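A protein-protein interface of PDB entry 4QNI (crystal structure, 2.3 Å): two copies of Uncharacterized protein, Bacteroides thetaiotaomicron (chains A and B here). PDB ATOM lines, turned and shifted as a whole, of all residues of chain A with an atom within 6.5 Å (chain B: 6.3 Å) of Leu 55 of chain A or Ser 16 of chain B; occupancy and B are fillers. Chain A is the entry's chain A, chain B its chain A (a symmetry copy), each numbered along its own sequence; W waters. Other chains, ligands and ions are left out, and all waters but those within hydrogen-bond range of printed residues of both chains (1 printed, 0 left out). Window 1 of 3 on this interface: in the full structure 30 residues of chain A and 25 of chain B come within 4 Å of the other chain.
The backbone carbonyl oxygen (O) of Ser 14 of chain B lies within hydrogen-bond range of the backbone NH (N) of Leu 55 of chain A (2.8 Å). ND2 of Asn 78 of chain B lies within hydrogen-bond range of OD1 of Asn 117 of chain A, 2.9 Å away. OG of Ser 57 of chain A is in hydrogen-bond range of N of Tyr 12 of chain B, 2.8 Å away. O of Tyr 158 of chain A sits at hydrogen-bond distance from N of Phe 15 of chain B, at 2.9 Å.
The backbone carbonyl oxygen (O) of Val 56 of chain A lies within hydrogen-bond range of the side-chain amide nitrogen (ND2) of Asn 117 of chain A (2.8 Å). The backbone carbonyl oxygen of Gly 119 of chain A lies within hydrogen-bond range of the backbone NH of Ile 54 of chain A, 2.9 Å away.
Among the printed residues, merely in contact across the chains: Val 56 of chain A with Ile 79 of chain B, Leu 55 of chain A with Ile 13 of chain B, Tyr 158 of chain A with Ser 14 of chain B, Val 56 of chain A with Tyr 12 of chain B, Tyr 158 of chain A with Ser 17 of chain B, Asn 117 of chain A with Ile 79 of chain B, Ile 54 of chain A with Ile 13 of chain B, Val 56 of chain A with Ile 13 of chain B, Pro 53 of chain A with Ser 16 of chain B, Pro 53 of chain A with Tyr 82 of chain B, Leu 55 of chain A with Tyr 12 of chain B, Leu 52 of chain A with Phe 15 of chain B, Ile 54 of chain A with Ser 14 of chain B, Tyr 158 of chain A with Gln 18 of chain B, Pro 53 of chain A with Phe 15 of chain B, Leu 55 of chain A with Ser 16 of chain B and Leu 55 of chain A with Ile 79 of chain B.
Of chain B, only Tyr 12, Ile 13, Ser 14, Ser 16 and Ile 79 come within 4 Å of Leu 55 of chain A. Of the printed residues of chain B, Asn 117 of chain A touches Asn 78 and Ile 79. Printed residues of chain B within 4 Å of Tyr 158 of chain A: Ser 14 (3.4 Å), Phe 15 (2.9 Å), Ser 17 (3.4 Å) and Gln 18 (3.7 Å). Of the printed residues of chain A, Ile 13 of chain B touches Ile 54, Leu 55 and Val 56. Of chain A, only Pro 53 (3.6 Å) and Leu 55 (3.9 Å) come within 4 Å of Ser 16 of chain B. Printed residues of chain A within 4 Å of Ser 17 of chain B: Tyr 158. Printed residues of chain A within 4 Å of Ile 79 of chain B: Leu 55 (3.96 Å), Val 56 (3.2 Å) and Asn 117 (3.5 Å). The nearest residue of chain B that does not touch Leu 55 of chain A is Tyr 82 of chain B (4.1 Å). The nearest printed residue of chain A that does not touch Gln 18 of chain B is Leu 55 of chain A (4.2 Å).
Of the 12 printed residues of chain A, 8 touch a printed residue of chain B. Hydrophobic or aromatic side chains of chain A that line the printed part of chain B: Leu 52, Pro 53, Ile 54, Leu 55, Val 56 and Tyr 158. Of the 11 printed residues of chain B, 10 touch a printed residue of chain A. Hydrophobic or aromatic side chains of chain B that line the printed part of chain A: Tyr 12, Ile 13, Phe 15, Ile 79 and Tyr 82. Among the printed residues, no Asp or Glu carboxylate lies within 4 Å of a Lys or Arg side-chain nitrogen of the other chain.
No position is printed for both chains. Of the 21 pairs that touch across the chains among the printed residues, none has its exchanged pair printed and touching as well.
Water W1 bridges O of Pro 53 of chain A (2.7 Å) and N of Ser 16 of chain B (2.7 Å).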
ATOM      1  N   THR A  25       4.648  -2.422  -5.612  1.00  0.00           N
ATOM      2  CA  THR A  25       3.291  -2.978  -5.607  1.00  0.00           C
ATOM      3  C   THR A  25       2.487  -2.259  -4.525  1.00  0.00           C
ATOM      4  O   THR A  25       2.917  -2.185  -3.384  1.00  0.00           O
ATOM      5  CB  THR A  25       3.295  -4.499  -5.366  1.00  0.00           C
ATOM      6  OG1 THR A  25       4.173  -5.124  -6.290  1.00  0.00           O
ATOM      7  CG2 THR A  25       1.915  -5.111  -5.474  1.00  0.00           C
ATOM      8  N   LEU A  52      -0.305 -12.229   2.629  1.00  0.00           N
ATOM      9  CA  LEU A  52       0.428 -12.081   1.373  1.00  0.00           C
ATOM     10  C   LEU A  52       0.695 -13.439   0.731  1.00  0.00           C
ATOM     11  O   LEU A  52       1.431 -14.251   1.294  1.00  0.00           O
ATOM     12  CB  LEU A  52       1.745 -11.307   1.629  1.00  0.00           C
ATOM     13  CG  LEU A  52       2.679 -11.047   0.442  1.00  0.00           C
ATOM     14  CD1 LEU A  52       2.139  -9.926  -0.453  1.00  0.00           C
ATOM     15  CD2 LEU A  52       4.077 -10.696   0.928  1.00  0.00           C
ATOM     16  N   PRO A  53       0.114 -13.697  -0.465  1.00  0.00           N
ATOM     17  CA  PRO A  53       0.332 -14.990  -1.126  1.00  0.00           C
ATOM     18  C   PRO A  53       1.758 -15.205  -1.621  1.00  0.00           C
ATOM     19  O   PRO A  53       2.416 -14.288  -2.110  1.00  0.00           O
ATOM     20  CB  PRO A  53      -0.630 -14.938  -2.318  1.00  0.00           C
ATOM     21  CG  PRO A  53      -1.630 -13.862  -1.978  1.00  0.00           C
ATOM     22  CD  PRO A  53      -0.814 -12.856  -1.255  1.00  0.00           C
ATOM     23  N   ILE A  54       2.222 -16.446  -1.478  1.00  0.00           N
ATOM     24  CA  ILE A  54       3.522 -16.934  -1.921  1.00  0.00           C
ATOM     25  C   ILE A  54       3.208 -18.158  -2.734  1.00  0.00           C
ATOM     26  O   ILE A  54       2.522 -19.064  -2.240  1.00  0.00           O
ATOM     27  CB  ILE A  54       4.486 -17.205  -0.740  1.00  0.00           C
ATOM     28  CG1 ILE A  54       4.945 -15.870  -0.072  1.00  0.00           C
ATOM     29  CG2 ILE A  54       5.670 -18.062  -1.195  1.00  0.00           C
ATOM     30  CD1 ILE A  54       5.829 -16.024   1.099  1.00  0.00           C
ATOM     31  N   LEU A  55       3.643 -18.154  -3.997  1.00  0.00           N
ATOM     32  CA  LEU A  55       3.376 -19.231  -4.936  1.00  0.00           C
ATOM     33  C   LEU A  55       4.550 -20.193  -5.037  1.00  0.00           C
ATOM     34  O   LEU A  55       5.710 -19.782  -5.007  1.00  0.00           O
ATOM     35  CB  LEU A  55       3.029 -18.640  -6.311  1.00  0.00           C
ATOM     36  CG  LEU A  55       1.900 -17.584  -6.362  1.00  0.00           C
ATOM     37  CD1 LEU A  55       1.850 -16.911  -7.738  1.00  0.00           C
ATOM     38  CD2 LEU A  55       0.552 -18.184  -5.999  1.00  0.00           C
ATOM     39  N   VAL A  56       4.236 -21.484  -5.121  1.00  0.00           N
ATOM     40  CA  VAL A  56       5.210 -22.580  -5.184  1.00  0.00           C
ATOM     41  C   VAL A  56       4.882 -23.519  -6.334  1.00  0.00           C
ATOM     42  O   VAL A  56       3.769 -24.025  -6.412  1.00  0.00           O
ATOM     43  CB  VAL A  56       5.260 -23.386  -3.853  1.00  0.00           C
ATOM     44  CG1 VAL A  56       6.460 -24.329  -3.829  1.00  0.00           C
ATOM     45  CG2 VAL A  56       5.264 -22.474  -2.628  1.00  0.00           C
ATOM     46  N   SER A  57       5.876 -23.805  -7.181  1.00  0.00           N
ATOM     47  CA  SER A  57       5.788 -24.790  -8.272  1.00  0.00           C
ATOM     48  C   SER A  57       6.185 -26.214  -7.743  1.00  0.00           C
ATOM     49  O   SER A  57       6.724 -26.325  -6.648  1.00  0.00           O
ATOM     50  CB  SER A  57       6.703 -24.370  -9.416  1.00  0.00           C
ATOM     51  OG  SER A  57       8.058 -24.423  -8.997  1.00  0.00           O
ATOM     52  N   ILE A 112       4.641 -24.584   3.629  1.00  0.00           N
ATOM     53  CA  ILE A 112       3.678 -24.863   2.556  1.00  0.00           C
ATOM     54  C   ILE A 112       3.349 -26.348   2.655  1.00  0.00           C
ATOM     55  O   ILE A 112       4.276 -27.166   2.676  1.00  0.00           O
ATOM     56  CB  ILE A 112       4.166 -24.464   1.113  1.00  0.00           C
ATOM     57  CG1 ILE A 112       4.956 -23.130   1.058  1.00  0.00           C
ATOM     58  CG2 ILE A 112       3.034 -24.525   0.077  1.00  0.00           C
ATOM     59  CD1 ILE A 112       4.194 -21.860   1.160  1.00  0.00           C
ATOM     60  N   ASN A 117       0.121 -25.321  -3.730  1.00  0.00           N
ATOM     61  CA  ASN A 117       0.895 -24.473  -4.637  1.00  0.00           C
ATOM     62  C   ASN A 117       0.957 -23.019  -4.126  1.00  0.00           C
ATOM     63  O   ASN A 117       1.530 -22.153  -4.784  1.00  0.00           O
ATOM     64  CB  ASN A 117       0.296 -24.541  -6.049  1.00  0.00           C
ATOM     65  CG  ASN A 117       0.645 -25.802  -6.784  1.00  0.00           C
ATOM     66  OD1 ASN A 117      -0.237 -26.598  -7.136  1.00  0.00           O
ATOM     67  ND2 ASN A 117       1.948 -26.058  -6.973  1.00  0.00           N
ATOM     68  N   LYS A 118       0.383 -22.772  -2.938  1.00  0.00           N
ATOM     69  CA  LYS A 118       0.336 -21.457  -2.304  1.00  0.00           C
ATOM     70  C   LYS A 118       0.463 -21.562  -0.795  1.00  0.00           C
ATOM     71  O   LYS A 118       0.203 -22.606  -0.204  1.00  0.00           O
ATOM     72  CB  LYS A 118      -0.974 -20.706  -2.665  1.00  0.00           C
ATOM     73  N   GLY A 119       0.876 -20.457  -0.205  1.00  0.00           N
ATOM     74  CA  GLY A 119       1.005 -20.227   1.228  1.00  0.00           C
ATOM     75  C   GLY A 119       0.703 -18.767   1.488  1.00  0.00           C
ATOM     76  O   GLY A 119       0.773 -17.946   0.570  1.00  0.00           O
ATOM     77  N   TYR A 158      10.167 -11.489  -9.439  1.00  0.00           N
ATOM     78  CA  TYR A 158       9.137 -12.388  -8.888  1.00  0.00           C
ATOM     79  C   TYR A 158       9.449 -12.832  -7.466  1.00  0.00           C
ATOM     80  O   TYR A 158       8.534 -13.094  -6.704  1.00  0.00           O
ATOM     81  CB  TYR A 158       8.976 -13.650  -9.766  1.00  0.00           C
ATOM     82  CG  TYR A 158       8.232 -13.489 -11.077  1.00  0.00           C
ATOM     83  CD1 TYR A 158       7.741 -12.251 -11.482  1.00  0.00           C
ATOM     84  CD2 TYR A 158       8.033 -14.576 -11.924  1.00  0.00           C
ATOM     85  CE1 TYR A 158       7.058 -12.100 -12.688  1.00  0.00           C
ATOM     86  CE2 TYR A 158       7.364 -14.436 -13.139  1.00  0.00           C
ATOM     87  CZ  TYR A 158       6.880 -13.196 -13.520  1.00  0.00           C
ATOM     88  OH  TYR A 158       6.221 -13.055 -14.721  1.00  0.00           O
ATOM     89  N   TYR B  12      10.208 -23.669  -7.400  1.00  0.00           N
ATOM     90  CA  TYR B  12      10.355 -22.244  -7.672  1.00  0.00           C
ATOM     91  C   TYR B  12       9.347 -21.488  -6.794  1.00  0.00           C
ATOM     92  O   TYR B  12       8.168 -21.834  -6.755  1.00  0.00           O
ATOM     93  CB  TYR B  12      10.133 -21.927  -9.158  1.00  0.00           C
ATOM     94  CG  TYR B  12      11.308 -22.120 -10.093  1.00  0.00           C
ATOM     95  CD1 TYR B  12      12.587 -22.376  -9.602  1.00  0.00           C
ATOM     96  CD2 TYR B  12      11.151 -22.005 -11.472  1.00  0.00           C
ATOM     97  CE1 TYR B  12      13.676 -22.536 -10.462  1.00  0.00           C
ATOM     98  CE2 TYR B  12      12.233 -22.148 -12.342  1.00  0.00           C
ATOM     99  CZ  TYR B  12      13.495 -22.419 -11.834  1.00  0.00           C
ATOM    100  OH  TYR B  12      14.560 -22.564 -12.696  1.00  0.00           O
ATOM    101  N   ILE B  13       9.836 -20.504  -6.045  1.00  0.00           N
ATOM    102  CA  ILE B  13       9.048 -19.687  -5.130  1.00  0.00           C
ATOM    103  C   ILE B  13       8.976 -18.262  -5.650  1.00  0.00           C
ATOM    104  O   ILE B  13       9.996 -17.696  -6.044  1.00  0.00           O
ATOM    105  CB  ILE B  13       9.663 -19.716  -3.708  1.00  0.00           C
ATOM    106  CG1 ILE B  13      10.169 -21.117  -3.268  1.00  0.00           C
ATOM    107  CG2 ILE B  13       8.740 -19.068  -2.698  1.00  0.00           C
ATOM    108  CD1 ILE B  13       9.138 -22.164  -2.858  1.00  0.00           C
ATOM    109  N   SER B  14       7.787 -17.668  -5.621  1.00  0.00           N
ATOM    110  CA  SER B  14       7.600 -16.278  -6.049  1.00  0.00           C
ATOM    111  C   SER B  14       6.389 -15.623  -5.359  1.00  0.00           C
ATOM    112  O   SER B  14       5.452 -16.317  -4.983  1.00  0.00           O
ATOM    113  CB  SER B  14       7.431 -16.202  -7.566  1.00  0.00           C
ATOM    114  OG  SER B  14       6.130 -16.606  -7.941  1.00  0.00           O
ATOM    115  N   PHE B  15       6.394 -14.293  -5.229  1.00  0.00           N
ATOM    116  CA  PHE B  15       5.258 -13.540  -4.682  1.00  0.00           C
ATOM    117  C   PHE B  15       4.247 -13.420  -5.782  1.00  0.00           C
ATOM    118  O   PHE B  15       4.693 -13.461  -6.910  1.00  0.00           O
ATOM    119  CB  PHE B  15       5.713 -12.161  -4.214  1.00  0.00           C
ATOM    120  CG  PHE B  15       6.635 -12.201  -3.041  1.00  0.00           C
ATOM    121  CD1 PHE B  15       6.135 -12.279  -1.747  1.00  0.00           C
ATOM    122  CD2 PHE B  15       8.005 -12.100  -3.213  1.00  0.00           C
ATOM    123  CE1 PHE B  15       6.987 -12.274  -0.655  1.00  0.00           C
ATOM    124  CE2 PHE B  15       8.857 -12.081  -2.118  1.00  0.00           C
ATOM    125  CZ  PHE B  15       8.345 -12.162  -0.843  1.00  0.00           C
ATOM    126  N   SER B  16       2.919 -13.252  -5.502  1.00  0.00           N
ATOM    127  CA  SER B  16       1.880 -13.140  -6.557  1.00  0.00           C
ATOM    128  C   SER B  16       2.225 -11.996  -7.556  1.00  0.00           C
ATOM    129  O   SER B  16       1.778 -10.834  -7.506  1.00  0.00           O
ATOM    130  CB  SER B  16       0.460 -13.026  -6.005  1.00  0.00           C
ATOM    131  OG  SER B  16      -0.415 -13.881  -6.729  1.00  0.00           O
ATOM    132  N   SER B  17       3.164 -12.421  -8.399  1.00  0.00           N
ATOM    133  CA  SER B  17       3.857 -11.895  -9.559  1.00  0.00           C
ATOM    134  C   SER B  17       4.162 -13.164 -10.364  1.00  0.00           C
ATOM    135  O   SER B  17       5.015 -13.984  -9.987  1.00  0.00           O
ATOM    136  CB  SER B  17       5.108 -11.114  -9.155  1.00  0.00           C
ATOM    137  OG  SER B  17       4.833 -10.168  -8.136  1.00  0.00           O
ATOM    138  N   GLN B  18       3.298 -13.415 -11.334  1.00  0.00           N
ATOM    139  CA  GLN B  18       3.374 -14.526 -12.257  1.00  0.00           C
ATOM    140  C   GLN B  18       2.840 -14.001 -13.586  1.00  0.00           C
ATOM    141  O   GLN B  18       1.859 -13.242 -13.589  1.00  0.00           O
ATOM    142  CB  GLN B  18       2.603 -15.748 -11.718  1.00  0.00           C
ATOM    143  N   ASN B  78      -2.991 -24.682 -11.044  1.00  0.00           N
ATOM    144  CA  ASN B  78      -3.218 -24.144  -9.698  1.00  0.00           C
ATOM    145  C   ASN B  78      -2.616 -22.751  -9.517  1.00  0.00           C
ATOM    146  O   ASN B  78      -3.326 -21.863  -9.053  1.00  0.00           O
ATOM    147  CB  ASN B  78      -2.678 -25.081  -8.642  1.00  0.00           C
ATOM    148  CG  ASN B  78      -3.520 -26.325  -8.499  1.00  0.00           C
ATOM    149  OD1 ASN B  78      -4.670 -26.384  -8.938  1.00  0.00           O
ATOM    150  ND2 ASN B  78      -2.951 -27.355  -7.908  1.00  0.00           N
ATOM    151  N   ILE B  79      -1.333 -22.544  -9.915  1.00  0.00           N
ATOM    152  CA  ILE B  79      -0.660 -21.227  -9.847  1.00  0.00           C
ATOM    153  C   ILE B  79      -1.487 -20.210 -10.646  1.00  0.00           C
ATOM    154  O   ILE B  79      -1.835 -19.151 -10.119  1.00  0.00           O
ATOM    155  CB  ILE B  79       0.811 -21.267 -10.345  1.00  0.00           C
ATOM    156  CG1 ILE B  79       1.666 -22.377  -9.692  1.00  0.00           C
ATOM    157  CG2 ILE B  79       1.490 -19.886 -10.322  1.00  0.00           C
ATOM    158  CD1 ILE B  79       1.894 -22.260  -8.288  1.00  0.00           C
ATOM    159  N   TYR B  82      -4.826 -19.291  -8.855  1.00  0.00           N
ATOM    160  CA  TYR B  82      -4.646 -18.403  -7.705  1.00  0.00           C
ATOM    161  C   TYR B  82      -4.183 -17.014  -8.140  1.00  0.00           C
ATOM    162  O   TYR B  82      -4.706 -16.021  -7.629  1.00  0.00           O
ATOM    163  CB  TYR B  82      -3.729 -18.974  -6.618  1.00  0.00           C
ATOM    164  CG  TYR B  82      -4.021 -18.322  -5.281  1.00  0.00           C
ATOM    165  CD1 TYR B  82      -5.081 -18.756  -4.484  1.00  0.00           C
ATOM    166  CD2 TYR B  82      -3.284 -17.220  -4.840  1.00  0.00           C
ATOM    167  CE1 TYR B  82      -5.378 -18.130  -3.267  1.00  0.00           C
ATOM    168  CE2 TYR B  82      -3.592 -16.572  -3.644  1.00  0.00           C
ATOM    169  CZ  TYR B  82      -4.624 -17.044  -2.847  1.00  0.00           C
ATOM    170  OH  TYR B  82      -4.917 -16.418  -1.654  1.00  0.00           O
ATOM    171  N   ALA B  83      -3.281 -16.942  -9.134  1.00  0.00           N
ATOM    172  CA  ALA B  83      -2.775 -15.677  -9.680  1.00  0.00           C
ATOM    173  C   ALA B  83      -3.874 -14.870 -10.370  1.00  0.00           C
ATOM    174  O   ALA B  83      -3.872 -13.647 -10.306  1.00  0.00           O
ATOM    175  CB  ALA B  83      -1.639 -15.941 -10.668  1.00  0.00           C
HETATM  176  O   HOH W   1       2.108 -11.910  -3.275  1.00  0.00           O
